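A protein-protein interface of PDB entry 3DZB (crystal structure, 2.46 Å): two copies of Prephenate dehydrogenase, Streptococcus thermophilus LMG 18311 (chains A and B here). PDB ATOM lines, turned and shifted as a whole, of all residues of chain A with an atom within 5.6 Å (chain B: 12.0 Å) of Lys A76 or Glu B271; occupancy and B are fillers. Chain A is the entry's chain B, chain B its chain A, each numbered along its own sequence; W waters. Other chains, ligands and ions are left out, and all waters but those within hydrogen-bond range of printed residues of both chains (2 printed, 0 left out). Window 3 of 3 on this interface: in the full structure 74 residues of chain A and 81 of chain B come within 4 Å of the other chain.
OE1 of Glu B271 lies within salt-bridge range of NZ of Lys A76.
Trp B275 touches Gly A235. Ala A238 touches Ile B274. CB of Ala A238 touches N of Trp B275, at 3.9 Å. CD2 of Phe B278 touches N of Ala A238, 3.8 Å away. Glu B271 touches Ser A239 (OE2 to CA, 3.6 Å). CE of Met A242 touches O of Glu B269 (3.7 Å). Glu B271 touches Met A242. Ile B274 touches Met A242 (CD1 to SD, 3.9 Å).
No residue of chain B comes within 4 Å of Pro A74. Of chain B, only Glu B271 comes within 4 Å of Lys A76. No residue of chain B comes within 4 Å of Gln A77. No residue of chain B comes within 4 Å of Ala A80. Gly A235 touches just one residue of chain B: Trp B275 (3.6 Å). Met A242 touches just these residues of chain B: Glu B269 (3.7 Å), Glu B271 (3.8 Å) and Ile B274 (3.9 Å). Asp B264 touches none of the printed residues of chain A. Ile B266 touches none of the printed residues of chain A. Printed residues of chain A within 4 Å of Glu B269: Met A242. Glu B271 touches just these residues of chain A: Lys A76, Ser A239 and Met A242. Printed residues of chain A within 4 Å of Ile B274: Ala A238 and Met A242. Printed residues of chain A within 4 Å of Trp B275: Gly A235 and Ala A238. Printed residues of chain A within 4 Å of Phe B278: Ala A238 (3.8 Å). The nearest residue of chain B that does not touch Lys A76 is Glu B269 (7.1 Å). The nearest residue of chain A that does not touch Glu B271 is Ala A238 (4.1 Å). The nearest printed residue of chain A that does not touch Phe B278 is Gly A235 (5.9 Å).
Of the 12 printed residues of chain A, 5 touch a printed residue of chain B. Printed residues of chain A that touch a printed residue of chain B: Lys A76, Gly A235, Ala A238, Ser A239 and Met A242. Hydrophobic or aromatic side chains of chain A within 4 Å of the printed part of chain B: Ala A238 and Met A242. Along chain A the printed residues that touch a printed residue of chain B span positions 76 to 242. Of the 20 printed residues of chain B, 5 touch a printed residue of chain A. Printed residues of chain B that touch a printed residue of chain A: Glu B269, Glu B271, Ile B274, Trp B275 and Phe B278. Hydrophobic or aromatic side chains of chain B within 4 Å of the printed part of chain A: Ile B274, Trp B275 and Phe B278. Among the printed residues, 9 pairs touch across the chains. Among the printed residues, Asp or Glu carboxylates within 4 Å of a Lys or Arg side-chain nitrogen of the other chain: Lys A76 with Glu B271.
No position is printed for both chains. Of the 9 pairs that touch across the chains among the printed residues, none has its exchanged pair printed and touching as well.
Water W2 bridges OE2 of Glu B271 and NZ of Lys A76. Water W1 lies within hydrogen-bond range of OE2 of Glu B271 and O of Gly A235.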
ATOM      1  N   PRO A  74     -11.793 -28.687 -17.575  1.00  0.00           N
ATOM      2  CA  PRO A  74     -11.343 -27.292 -17.559  1.00  0.00           C
ATOM      3  C   PRO A  74     -11.999 -26.474 -16.458  1.00  0.00           C
ATOM      4  O   PRO A  74     -13.110 -26.755 -16.038  1.00  0.00           O
ATOM      5  CB  PRO A  74     -11.711 -26.797 -18.949  1.00  0.00           C
ATOM      6  CG  PRO A  74     -11.563 -28.031 -19.793  1.00  0.00           C
ATOM      7  CD  PRO A  74     -12.187 -29.107 -18.932  1.00  0.00           C
ATOM      8  N   ILE A  75     -11.290 -25.449 -16.003  1.00  0.00           N
ATOM      9  CA  ILE A  75     -11.763 -24.566 -14.950  1.00  0.00           C
ATOM     10  C   ILE A  75     -13.209 -24.145 -15.161  1.00  0.00           C
ATOM     11  O   ILE A  75     -14.021 -24.249 -14.251  1.00  0.00           O
ATOM     12  CB  ILE A  75     -10.854 -23.314 -14.849  1.00  0.00           C
ATOM     13  CG1 ILE A  75      -9.428 -23.754 -14.495  1.00  0.00           C
ATOM     14  CG2 ILE A  75     -11.382 -22.342 -13.788  1.00  0.00           C
ATOM     15  CD1 ILE A  75      -8.418 -22.627 -14.453  1.00  0.00           C
ATOM     16  N   LYS A  76     -13.542 -23.687 -16.360  1.00  0.00           N
ATOM     17  CA  LYS A  76     -14.907 -23.253 -16.634  1.00  0.00           C
ATOM     18  C   LYS A  76     -15.917 -24.368 -16.335  1.00  0.00           C
ATOM     19  O   LYS A  76     -16.927 -24.145 -15.657  1.00  0.00           O
ATOM     20  CB  LYS A  76     -15.038 -22.801 -18.088  1.00  0.00           C
ATOM     21  CG  LYS A  76     -16.258 -21.923 -18.347  1.00  0.00           C
ATOM     22  CD  LYS A  76     -16.068 -20.513 -17.784  1.00  0.00           C
ATOM     23  CE  LYS A  76     -15.018 -19.720 -18.587  1.00  0.00           C
ATOM     24  NZ  LYS A  76     -14.769 -18.329 -18.053  1.00  0.00           N
ATOM     25  N   GLN A  77     -15.636 -25.567 -16.842  1.00  0.00           N
ATOM     26  CA  GLN A  77     -16.506 -26.724 -16.624  1.00  0.00           C
ATOM     27  C   GLN A  77     -16.566 -27.100 -15.155  1.00  0.00           C
ATOM     28  O   GLN A  77     -17.600 -27.520 -14.653  1.00  0.00           O
ATOM     29  CB  GLN A  77     -16.003 -27.935 -17.410  1.00  0.00           C
ATOM     30  CG  GLN A  77     -16.875 -28.332 -18.573  1.00  0.00           C
ATOM     31  CD  GLN A  77     -18.308 -28.610 -18.154  1.00  0.00           C
ATOM     32  OE1 GLN A  77     -19.176 -28.878 -18.991  1.00  0.00           O
ATOM     33  NE2 GLN A  77     -18.565 -28.553 -16.852  1.00  0.00           N
ATOM     34  N   THR A  78     -15.448 -26.944 -14.460  1.00  0.00           N
ATOM     35  CA  THR A  78     -15.399 -27.300 -13.056  1.00  0.00           C
ATOM     36  C   THR A  78     -16.389 -26.492 -12.221  1.00  0.00           C
ATOM     37  O   THR A  78     -17.079 -27.031 -11.365  1.00  0.00           O
ATOM     38  CB  THR A  78     -13.980 -27.124 -12.498  1.00  0.00           C
ATOM     39  OG1 THR A  78     -13.086 -27.999 -13.196  1.00  0.00           O
ATOM     40  CG2 THR A  78     -13.942 -27.464 -11.022  1.00  0.00           C
ATOM     41  N   MET A  79     -16.468 -25.196 -12.466  1.00  0.00           N
ATOM     42  CA  MET A  79     -17.396 -24.386 -11.703  1.00  0.00           C
ATOM     43  C   MET A  79     -18.836 -24.668 -12.120  1.00  0.00           C
ATOM     44  O   MET A  79     -19.741 -24.640 -11.296  1.00  0.00           O
ATOM     45  CB  MET A  79     -17.042 -22.909 -11.858  1.00  0.00           C
ATOM     46  CG  MET A  79     -15.676 -22.598 -11.265  1.00  0.00           C
ATOM     47  SD  MET A  79     -15.095 -20.763 -11.421  1.00  0.00           S
ATOM     48  CE  MET A  79     -15.062 -20.626 -13.347  1.00  0.00           C
ATOM     49  N   ALA A  80     -19.034 -24.958 -13.401  1.00  0.00           N
ATOM     50  CA  ALA A  80     -20.359 -25.274 -13.913  1.00  0.00           C
ATOM     51  C   ALA A  80     -20.861 -26.523 -13.198  1.00  0.00           C
ATOM     52  O   ALA A  80     -22.002 -26.570 -12.731  1.00  0.00           O
ATOM     53  CB  ALA A  80     -20.296 -25.530 -15.402  1.00  0.00           C
ATOM     54  N   TYR A  81     -19.997 -27.535 -13.112  1.00  0.00           N
ATOM     55  CA  TYR A  81     -20.348 -28.782 -12.450  1.00  0.00           C
ATOM     56  C   TYR A  81     -20.529 -28.587 -10.946  1.00  0.00           C
ATOM     57  O   TYR A  81     -21.332 -29.278 -10.324  1.00  0.00           O
ATOM     58  CB  TYR A  81     -19.283 -29.856 -12.708  1.00  0.00           C
ATOM     59  CG  TYR A  81     -19.292 -30.456 -14.106  1.00  0.00           C
ATOM     60  CD1 TYR A  81     -20.477 -30.578 -14.831  1.00  0.00           C
ATOM     61  CD2 TYR A  81     -18.122 -30.957 -14.676  1.00  0.00           C
ATOM     62  CE1 TYR A  81     -20.492 -31.186 -16.088  1.00  0.00           C
ATOM     63  CE2 TYR A  81     -18.128 -31.566 -15.927  1.00  0.00           C
ATOM     64  CZ  TYR A  81     -19.315 -31.676 -16.626  1.00  0.00           C
ATOM     65  OH  TYR A  81     -19.321 -32.270 -17.866  1.00  0.00           O
ATOM     66  N   GLY A 235      -6.087 -23.399 -24.837  1.00  0.00           N
ATOM     67  CA  GLY A 235      -7.281 -23.354 -24.019  1.00  0.00           C
ATOM     68  C   GLY A 235      -7.025 -23.218 -22.534  1.00  0.00           C
ATOM     69  O   GLY A 235      -7.449 -22.254 -21.893  1.00  0.00           O
ATOM     70  N   ALA A 238      -5.542 -19.966 -21.443  1.00  0.00           N
ATOM     71  CA  ALA A 238      -6.462 -18.852 -21.571  1.00  0.00           C
ATOM     72  C   ALA A 238      -7.359 -18.873 -20.331  1.00  0.00           C
ATOM     73  O   ALA A 238      -7.592 -17.843 -19.707  1.00  0.00           O
ATOM     74  CB  ALA A 238      -7.303 -19.003 -22.819  1.00  0.00           C
ATOM     75  N   SER A 239      -7.840 -20.058 -19.966  1.00  0.00           N
ATOM     76  CA  SER A 239      -8.714 -20.196 -18.804  1.00  0.00           C
ATOM     77  C   SER A 239      -7.983 -19.830 -17.511  1.00  0.00           C
ATOM     78  O   SER A 239      -8.581 -19.266 -16.594  1.00  0.00           O
ATOM     79  CB  SER A 239      -9.248 -21.624 -18.708  1.00  0.00           C
ATOM     80  OG  SER A 239      -8.258 -22.517 -18.232  1.00  0.00           O
ATOM     81  N   MET A 242      -7.734 -16.144 -17.208  1.00  0.00           N
ATOM     82  CA  MET A 242      -9.060 -15.615 -16.934  1.00  0.00           C
ATOM     83  C   MET A 242      -9.419 -15.679 -15.447  1.00  0.00           C
ATOM     84  O   MET A 242     -10.008 -14.742 -14.901  1.00  0.00           O
ATOM     85  CB  MET A 242     -10.102 -16.378 -17.751  1.00  0.00           C
ATOM     86  CG  MET A 242     -10.114 -16.032 -19.233  1.00  0.00           C
ATOM     87  SD  MET A 242     -10.807 -14.243 -19.554  1.00  0.00           S
ATOM     88  CE  MET A 242     -12.582 -14.499 -18.805  1.00  0.00           C
ATOM     89  N   HIS B 261      -1.345  -5.105 -24.049  1.00  0.00           N
ATOM     90  CA  HIS B 261      -2.423  -5.674 -24.843  1.00  0.00           C
ATOM     91  C   HIS B 261      -3.081  -6.829 -24.098  1.00  0.00           C
ATOM     92  O   HIS B 261      -4.299  -6.838 -23.914  1.00  0.00           O
ATOM     93  CB  HIS B 261      -1.907  -6.187 -26.180  1.00  0.00           C
ATOM     94  CG  HIS B 261      -2.960  -6.853 -27.008  1.00  0.00           C
ATOM     95  ND1 HIS B 261      -2.781  -8.089 -27.586  1.00  0.00           N
ATOM     96  CD2 HIS B 261      -4.210  -6.456 -27.346  1.00  0.00           C
ATOM     97  CE1 HIS B 261      -3.875  -8.428 -28.247  1.00  0.00           C
ATOM     98  NE2 HIS B 261      -4.757  -7.454 -28.116  1.00  0.00           N
ATOM     99  N   VAL B 262      -2.266  -7.802 -23.681  1.00  0.00           N
ATOM    100  CA  VAL B 262      -2.749  -8.972 -22.952  1.00  0.00           C
ATOM    101  C   VAL B 262      -3.496  -8.525 -21.701  1.00  0.00           C
ATOM    102  O   VAL B 262      -4.573  -9.036 -21.384  1.00  0.00           O
ATOM    103  CB  VAL B 262      -1.573  -9.892 -22.560  1.00  0.00           C
ATOM    104  CG1 VAL B 262      -2.063 -11.038 -21.691  1.00  0.00           C
ATOM    105  CG2 VAL B 262      -0.915 -10.442 -23.809  1.00  0.00           C
ATOM    106  N   ALA B 263      -2.929  -7.552 -20.999  1.00  0.00           N
ATOM    107  CA  ALA B 263      -3.556  -7.032 -19.797  1.00  0.00           C
ATOM    108  C   ALA B 263      -4.907  -6.427 -20.155  1.00  0.00           C
ATOM    109  O   ALA B 263      -5.835  -6.435 -19.347  1.00  0.00           O
ATOM    110  CB  ALA B 263      -2.675  -5.989 -19.161  1.00  0.00           C
ATOM    111  N   ASP B 264      -5.020  -5.887 -21.361  1.00  0.00           N
ATOM    112  CA  ASP B 264      -6.285  -5.301 -21.782  1.00  0.00           C
ATOM    113  C   ASP B 264      -7.281  -6.432 -21.961  1.00  0.00           C
ATOM    114  O   ASP B 264      -8.402  -6.359 -21.460  1.00  0.00           O
ATOM    115  CB  ASP B 264      -6.125  -4.533 -23.096  1.00  0.00           C
ATOM    116  CG  ASP B 264      -5.481  -3.179 -22.902  1.00  0.00           C
ATOM    117  OD1 ASP B 264      -5.090  -2.571 -23.923  1.00  0.00           O
ATOM    118  OD2 ASP B 264      -5.371  -2.718 -21.742  1.00  0.00           O
ATOM    119  N   LEU B 265      -6.848  -7.472 -22.677  1.00  0.00           N
ATOM    120  CA  LEU B 265      -7.656  -8.657 -22.932  1.00  0.00           C
ATOM    121  C   LEU B 265      -8.167  -9.278 -21.624  1.00  0.00           C
ATOM    122  O   LEU B 265      -9.312  -9.718 -21.546  1.00  0.00           O
ATOM    123  CB  LEU B 265      -6.837  -9.689 -23.714  1.00  0.00           C
ATOM    124  CG  LEU B 265      -6.884  -9.684 -25.249  1.00  0.00           C
ATOM    125  CD1 LEU B 265      -6.925  -8.274 -25.790  1.00  0.00           C
ATOM    126  CD2 LEU B 265      -5.675 -10.446 -25.781  1.00  0.00           C
ATOM    127  N   ILE B 266      -7.318  -9.308 -20.601  1.00  0.00           N
ATOM    128  CA  ILE B 266      -7.717  -9.867 -19.310  1.00  0.00           C
ATOM    129  C   ILE B 266      -8.780  -8.991 -18.671  1.00  0.00           C
ATOM    130  O   ILE B 266      -9.806  -9.481 -18.192  1.00  0.00           O
ATOM    131  CB  ILE B 266      -6.523  -9.973 -18.335  1.00  0.00           C
ATOM    132  CG1 ILE B 266      -5.627 -11.139 -18.737  1.00  0.00           C
ATOM    133  CG2 ILE B 266      -7.020 -10.151 -16.921  1.00  0.00           C
ATOM    134  CD1 ILE B 266      -4.335 -11.203 -17.962  1.00  0.00           C
ATOM    135  N   LYS B 267      -8.538  -7.690 -18.657  1.00  0.00           N
ATOM    136  CA  LYS B 267      -9.512  -6.791 -18.061  1.00  0.00           C
ATOM    137  C   LYS B 267     -10.832  -6.858 -18.820  1.00  0.00           C
ATOM    138  O   LYS B 267     -11.896  -6.714 -18.225  1.00  0.00           O
ATOM    139  CB  LYS B 267      -8.989  -5.362 -18.061  1.00  0.00           C
ATOM    140  CG  LYS B 267      -7.705  -5.161 -17.274  1.00  0.00           C
ATOM    141  CD  LYS B 267      -7.201  -3.750 -17.507  1.00  0.00           C
ATOM    142  CE  LYS B 267      -5.841  -3.523 -16.900  1.00  0.00           C
ATOM    143  NZ  LYS B 267      -5.195  -2.319 -17.503  1.00  0.00           N
ATOM    144  N   ALA B 268     -10.750  -7.096 -20.128  1.00  0.00           N
ATOM    145  CA  ALA B 268     -11.928  -7.184 -20.980  1.00  0.00           C
ATOM    146  C   ALA B 268     -12.621  -8.542 -20.892  1.00  0.00           C
ATOM    147  O   ALA B 268     -13.690  -8.733 -21.470  1.00  0.00           O
ATOM    148  CB  ALA B 268     -11.543  -6.904 -22.426  1.00  0.00           C
ATOM    149  N   GLU B 269     -12.002  -9.481 -20.178  1.00  0.00           N
ATOM    150  CA  GLU B 269     -12.532 -10.833 -20.024  1.00  0.00           C
ATOM    151  C   GLU B 269     -12.732 -11.482 -21.400  1.00  0.00           C
ATOM    152  O   GLU B 269     -13.616 -12.321 -21.596  1.00  0.00           O
ATOM    153  CB  GLU B 269     -13.852 -10.795 -19.247  1.00  0.00           C
ATOM    154  CG  GLU B 269     -13.837  -9.818 -18.077  1.00  0.00           C
ATOM    155  CD  GLU B 269     -14.678 -10.285 -16.908  1.00  0.00           C
ATOM    156  OE1 GLU B 269     -15.543 -11.166 -17.112  1.00  0.00           O
ATOM    157  OE2 GLU B 269     -14.479  -9.767 -15.787  1.00  0.00           O
ATOM    158  N   ASP B 270     -11.890 -11.090 -22.347  1.00  0.00           N
ATOM    159  CA  ASP B 270     -11.961 -11.612 -23.699  1.00  0.00           C
ATOM    160  C   ASP B 270     -11.204 -12.932 -23.827  1.00  0.00           C
ATOM    161  O   ASP B 270     -10.150 -13.000 -24.454  1.00  0.00           O
ATOM    162  CB  ASP B 270     -11.393 -10.581 -24.674  1.00  0.00           C
ATOM    163  CG  ASP B 270     -11.650 -10.942 -26.111  1.00  0.00           C
ATOM    164  OD1 ASP B 270     -11.354 -10.102 -26.982  1.00  0.00           O
ATOM    165  OD2 ASP B 270     -12.140 -12.063 -26.370  1.00  0.00           O
ATOM    166  N   GLU B 271     -11.762 -13.982 -23.234  1.00  0.00           N
ATOM    167  CA  GLU B 271     -11.149 -15.306 -23.266  1.00  0.00           C
ATOM    168  C   GLU B 271     -10.780 -15.803 -24.662  1.00  0.00           C
ATOM    169  O   GLU B 271      -9.773 -16.485 -24.829  1.00  0.00           O
ATOM    170  CB  GLU B 271     -12.071 -16.319 -22.585  1.00  0.00           C
ATOM    171  CG  GLU B 271     -11.570 -17.762 -22.599  1.00  0.00           C
ATOM    172  CD  GLU B 271     -12.282 -18.639 -21.566  1.00  0.00           C
ATOM    173  OE1 GLU B 271     -13.529 -18.571 -21.488  1.00  0.00           O
ATOM    174  OE2 GLU B 271     -11.600 -19.398 -20.836  1.00  0.00           O
ATOM    175  N   SER B 272     -11.579 -15.469 -25.664  1.00  0.00           N
ATOM    176  CA  SER B 272     -11.284 -15.911 -27.018  1.00  0.00           C
ATOM    177  C   SER B 272     -10.069 -15.212 -27.589  1.00  0.00           C
ATOM    178  O   SER B 272      -9.281 -15.827 -28.298  1.00  0.00           O
ATOM    179  CB  SER B 272     -12.484 -15.679 -27.933  1.00  0.00           C
ATOM    180  OG  SER B 272     -13.566 -16.500 -27.536  1.00  0.00           O
ATOM    181  N   ALA B 273      -9.917 -13.925 -27.298  1.00  0.00           N
ATOM    182  CA  ALA B 273      -8.757 -13.194 -27.800  1.00  0.00           C
ATOM    183  C   ALA B 273      -7.516 -13.743 -27.095  1.00  0.00           C
ATOM    184  O   ALA B 273      -6.442 -13.831 -27.700  1.00  0.00           O
ATOM    185  CB  ALA B 273      -8.905 -11.699 -27.531  1.00  0.00           C
ATOM    186  N   ILE B 274      -7.677 -14.113 -25.820  1.00  0.00           N
ATOM    187  CA  ILE B 274      -6.579 -14.674 -25.046  1.00  0.00           C
ATOM    188  C   ILE B 274      -6.227 -16.049 -25.604  1.00  0.00           C
ATOM    189  O   ILE B 274      -5.056 -16.410 -25.661  1.00  0.00           O
ATOM    190  CB  ILE B 274      -6.933 -14.766 -23.553  1.00  0.00           C
ATOM    191  CG1 ILE B 274      -7.244 -13.360 -23.020  1.00  0.00           C
ATOM    192  CG2 ILE B 274      -5.768 -15.355 -22.775  1.00  0.00           C
ATOM    193  CD1 ILE B 274      -7.630 -13.299 -21.572  1.00  0.00           C
ATOM    194  N   TRP B 275      -7.226 -16.809 -26.042  1.00  0.00           N
ATOM    195  CA  TRP B 275      -6.944 -18.113 -26.623  1.00  0.00           C
ATOM    196  C   TRP B 275      -6.063 -17.865 -27.842  1.00  0.00           C
ATOM    197  O   TRP B 275      -5.072 -18.561 -28.068  1.00  0.00           O
ATOM    198  CB  TRP B 275      -8.225 -18.823 -27.091  1.00  0.00           C
ATOM    199  CG  TRP B 275      -7.934 -20.113 -27.847  1.00  0.00           C
ATOM    200  CD1 TRP B 275      -7.732 -21.348 -27.307  1.00  0.00           C
ATOM    201  CD2 TRP B 275      -7.705 -20.258 -29.264  1.00  0.00           C
ATOM    202  NE1 TRP B 275      -7.385 -22.251 -28.289  1.00  0.00           N
ATOM    203  CE2 TRP B 275      -7.361 -21.611 -29.498  1.00  0.00           C
ATOM    204  CE3 TRP B 275      -7.751 -19.377 -30.355  1.00  0.00           C
ATOM    205  CZ2 TRP B 275      -7.063 -22.106 -30.778  1.00  0.00           C
ATOM    206  CZ3 TRP B 275      -7.453 -19.871 -31.634  1.00  0.00           C
ATOM    207  CH2 TRP B 275      -7.114 -21.225 -31.829  1.00  0.00           C
ATOM    208  N   GLU B 276      -6.453 -16.866 -28.623  1.00  0.00           N
ATOM    209  CA  GLU B 276      -5.751 -16.491 -29.846  1.00  0.00           C
ATOM    210  C   GLU B 276      -4.272 -16.198 -29.560  1.00  0.00           C
ATOM    211  O   GLU B 276      -3.377 -16.702 -30.242  1.00  0.00           O
ATOM    212  CB  GLU B 276      -6.434 -15.258 -30.460  1.00  0.00           C
ATOM    213  CG  GLU B 276      -5.990 -14.899 -31.867  1.00  0.00           C
ATOM    214  CD  GLU B 276      -6.742 -15.661 -32.967  1.00  0.00           C
ATOM    215  OE1 GLU B 276      -6.238 -15.658 -34.116  1.00  0.00           O
ATOM    216  OE2 GLU B 276      -7.831 -16.248 -32.703  1.00  0.00           O
ATOM    217  N   PHE B 277      -4.027 -15.385 -28.538  1.00  0.00           N
ATOM    218  CA  PHE B 277      -2.671 -15.012 -28.143  1.00  0.00           C
ATOM    219  C   PHE B 277      -1.793 -16.241 -27.922  1.00  0.00           C
ATOM    220  O   PHE B 277      -0.733 -16.380 -28.542  1.00  0.00           O
ATOM    221  CB  PHE B 277      -2.725 -14.181 -26.864  1.00  0.00           C
ATOM    222  CG  PHE B 277      -1.381 -13.953 -26.224  1.00  0.00           C
ATOM    223  CD1 PHE B 277      -0.413 -13.167 -26.846  1.00  0.00           C
ATOM    224  CD2 PHE B 277      -1.104 -14.480 -24.968  1.00  0.00           C
ATOM    225  CE1 PHE B 277       0.807 -12.902 -26.221  1.00  0.00           C
ATOM    226  CE2 PHE B 277       0.116 -14.220 -24.333  1.00  0.00           C
ATOM    227  CZ  PHE B 277       1.071 -13.427 -24.961  1.00  0.00           C
ATOM    228  N   PHE B 278      -2.238 -17.127 -27.037  1.00  0.00           N
ATOM    229  CA  PHE B 278      -1.497 -18.346 -26.734  1.00  0.00           C
ATOM    230  C   PHE B 278      -1.415 -19.299 -27.913  1.00  0.00           C
ATOM    231  O   PHE B 278      -0.427 -20.014 -28.063  1.00  0.00           O
ATOM    232  CB  PHE B 278      -2.113 -19.070 -25.543  1.00  0.00           C
ATOM    233  CG  PHE B 278      -1.864 -18.394 -24.229  1.00  0.00           C
ATOM    234  CD1 PHE B 278      -0.563 -18.185 -23.774  1.00  0.00           C
ATOM    235  CD2 PHE B 278      -2.928 -17.988 -23.429  1.00  0.00           C
ATOM    236  CE1 PHE B 278      -0.326 -17.583 -22.534  1.00  0.00           C
ATOM    237  CE2 PHE B 278      -2.704 -17.387 -22.190  1.00  0.00           C
ATOM    238  CZ  PHE B 278      -1.398 -17.186 -21.740  1.00  0.00           C
ATOM    239  N   ASP B 279      -2.443 -19.319 -28.753  1.00  0.00           N
ATOM    240  CA  ASP B 279      -2.408 -20.205 -29.905  1.00  0.00           C
ATOM    241  C   ASP B 279      -1.410 -19.682 -30.934  1.00  0.00           C
ATOM    242  O   ASP B 279      -0.687 -20.453 -31.557  1.00  0.00           O
ATOM    243  CB  ASP B 279      -3.789 -20.337 -30.538  1.00  0.00           C
ATOM    244  CG  ASP B 279      -3.805 -21.352 -31.666  1.00  0.00           C
ATOM    245  OD1 ASP B 279      -3.548 -22.540 -31.384  1.00  0.00           O
ATOM    246  OD2 ASP B 279      -4.060 -20.960 -32.831  1.00  0.00           O
ATOM    247  N   ASN B 280      -1.384 -18.368 -31.117  1.00  0.00           N
ATOM    248  CA  ASN B 280      -0.441 -17.747 -32.040  1.00  0.00           C
ATOM    249  C   ASN B 280       0.972 -18.130 -31.604  1.00  0.00           C
ATOM    250  O   ASN B 280       1.802 -18.532 -32.418  1.00  0.00           O
ATOM    251  CB  ASN B 280      -0.590 -16.222 -32.002  1.00  0.00           C
ATOM    252  CG  ASN B 280       0.570 -15.497 -32.685  1.00  0.00           C
ATOM    253  OD1 ASN B 280       0.757 -15.606 -33.896  1.00  0.00           O
ATOM    254  ND2 ASN B 280       1.356 -14.757 -31.902  1.00  0.00           N
HETATM  255  O   HOH W   1     -10.521 -21.551 -22.354  1.00  0.00           O
HETATM  256  O   HOH W   2     -12.117 -20.570 -18.334  1.00  0.00           O
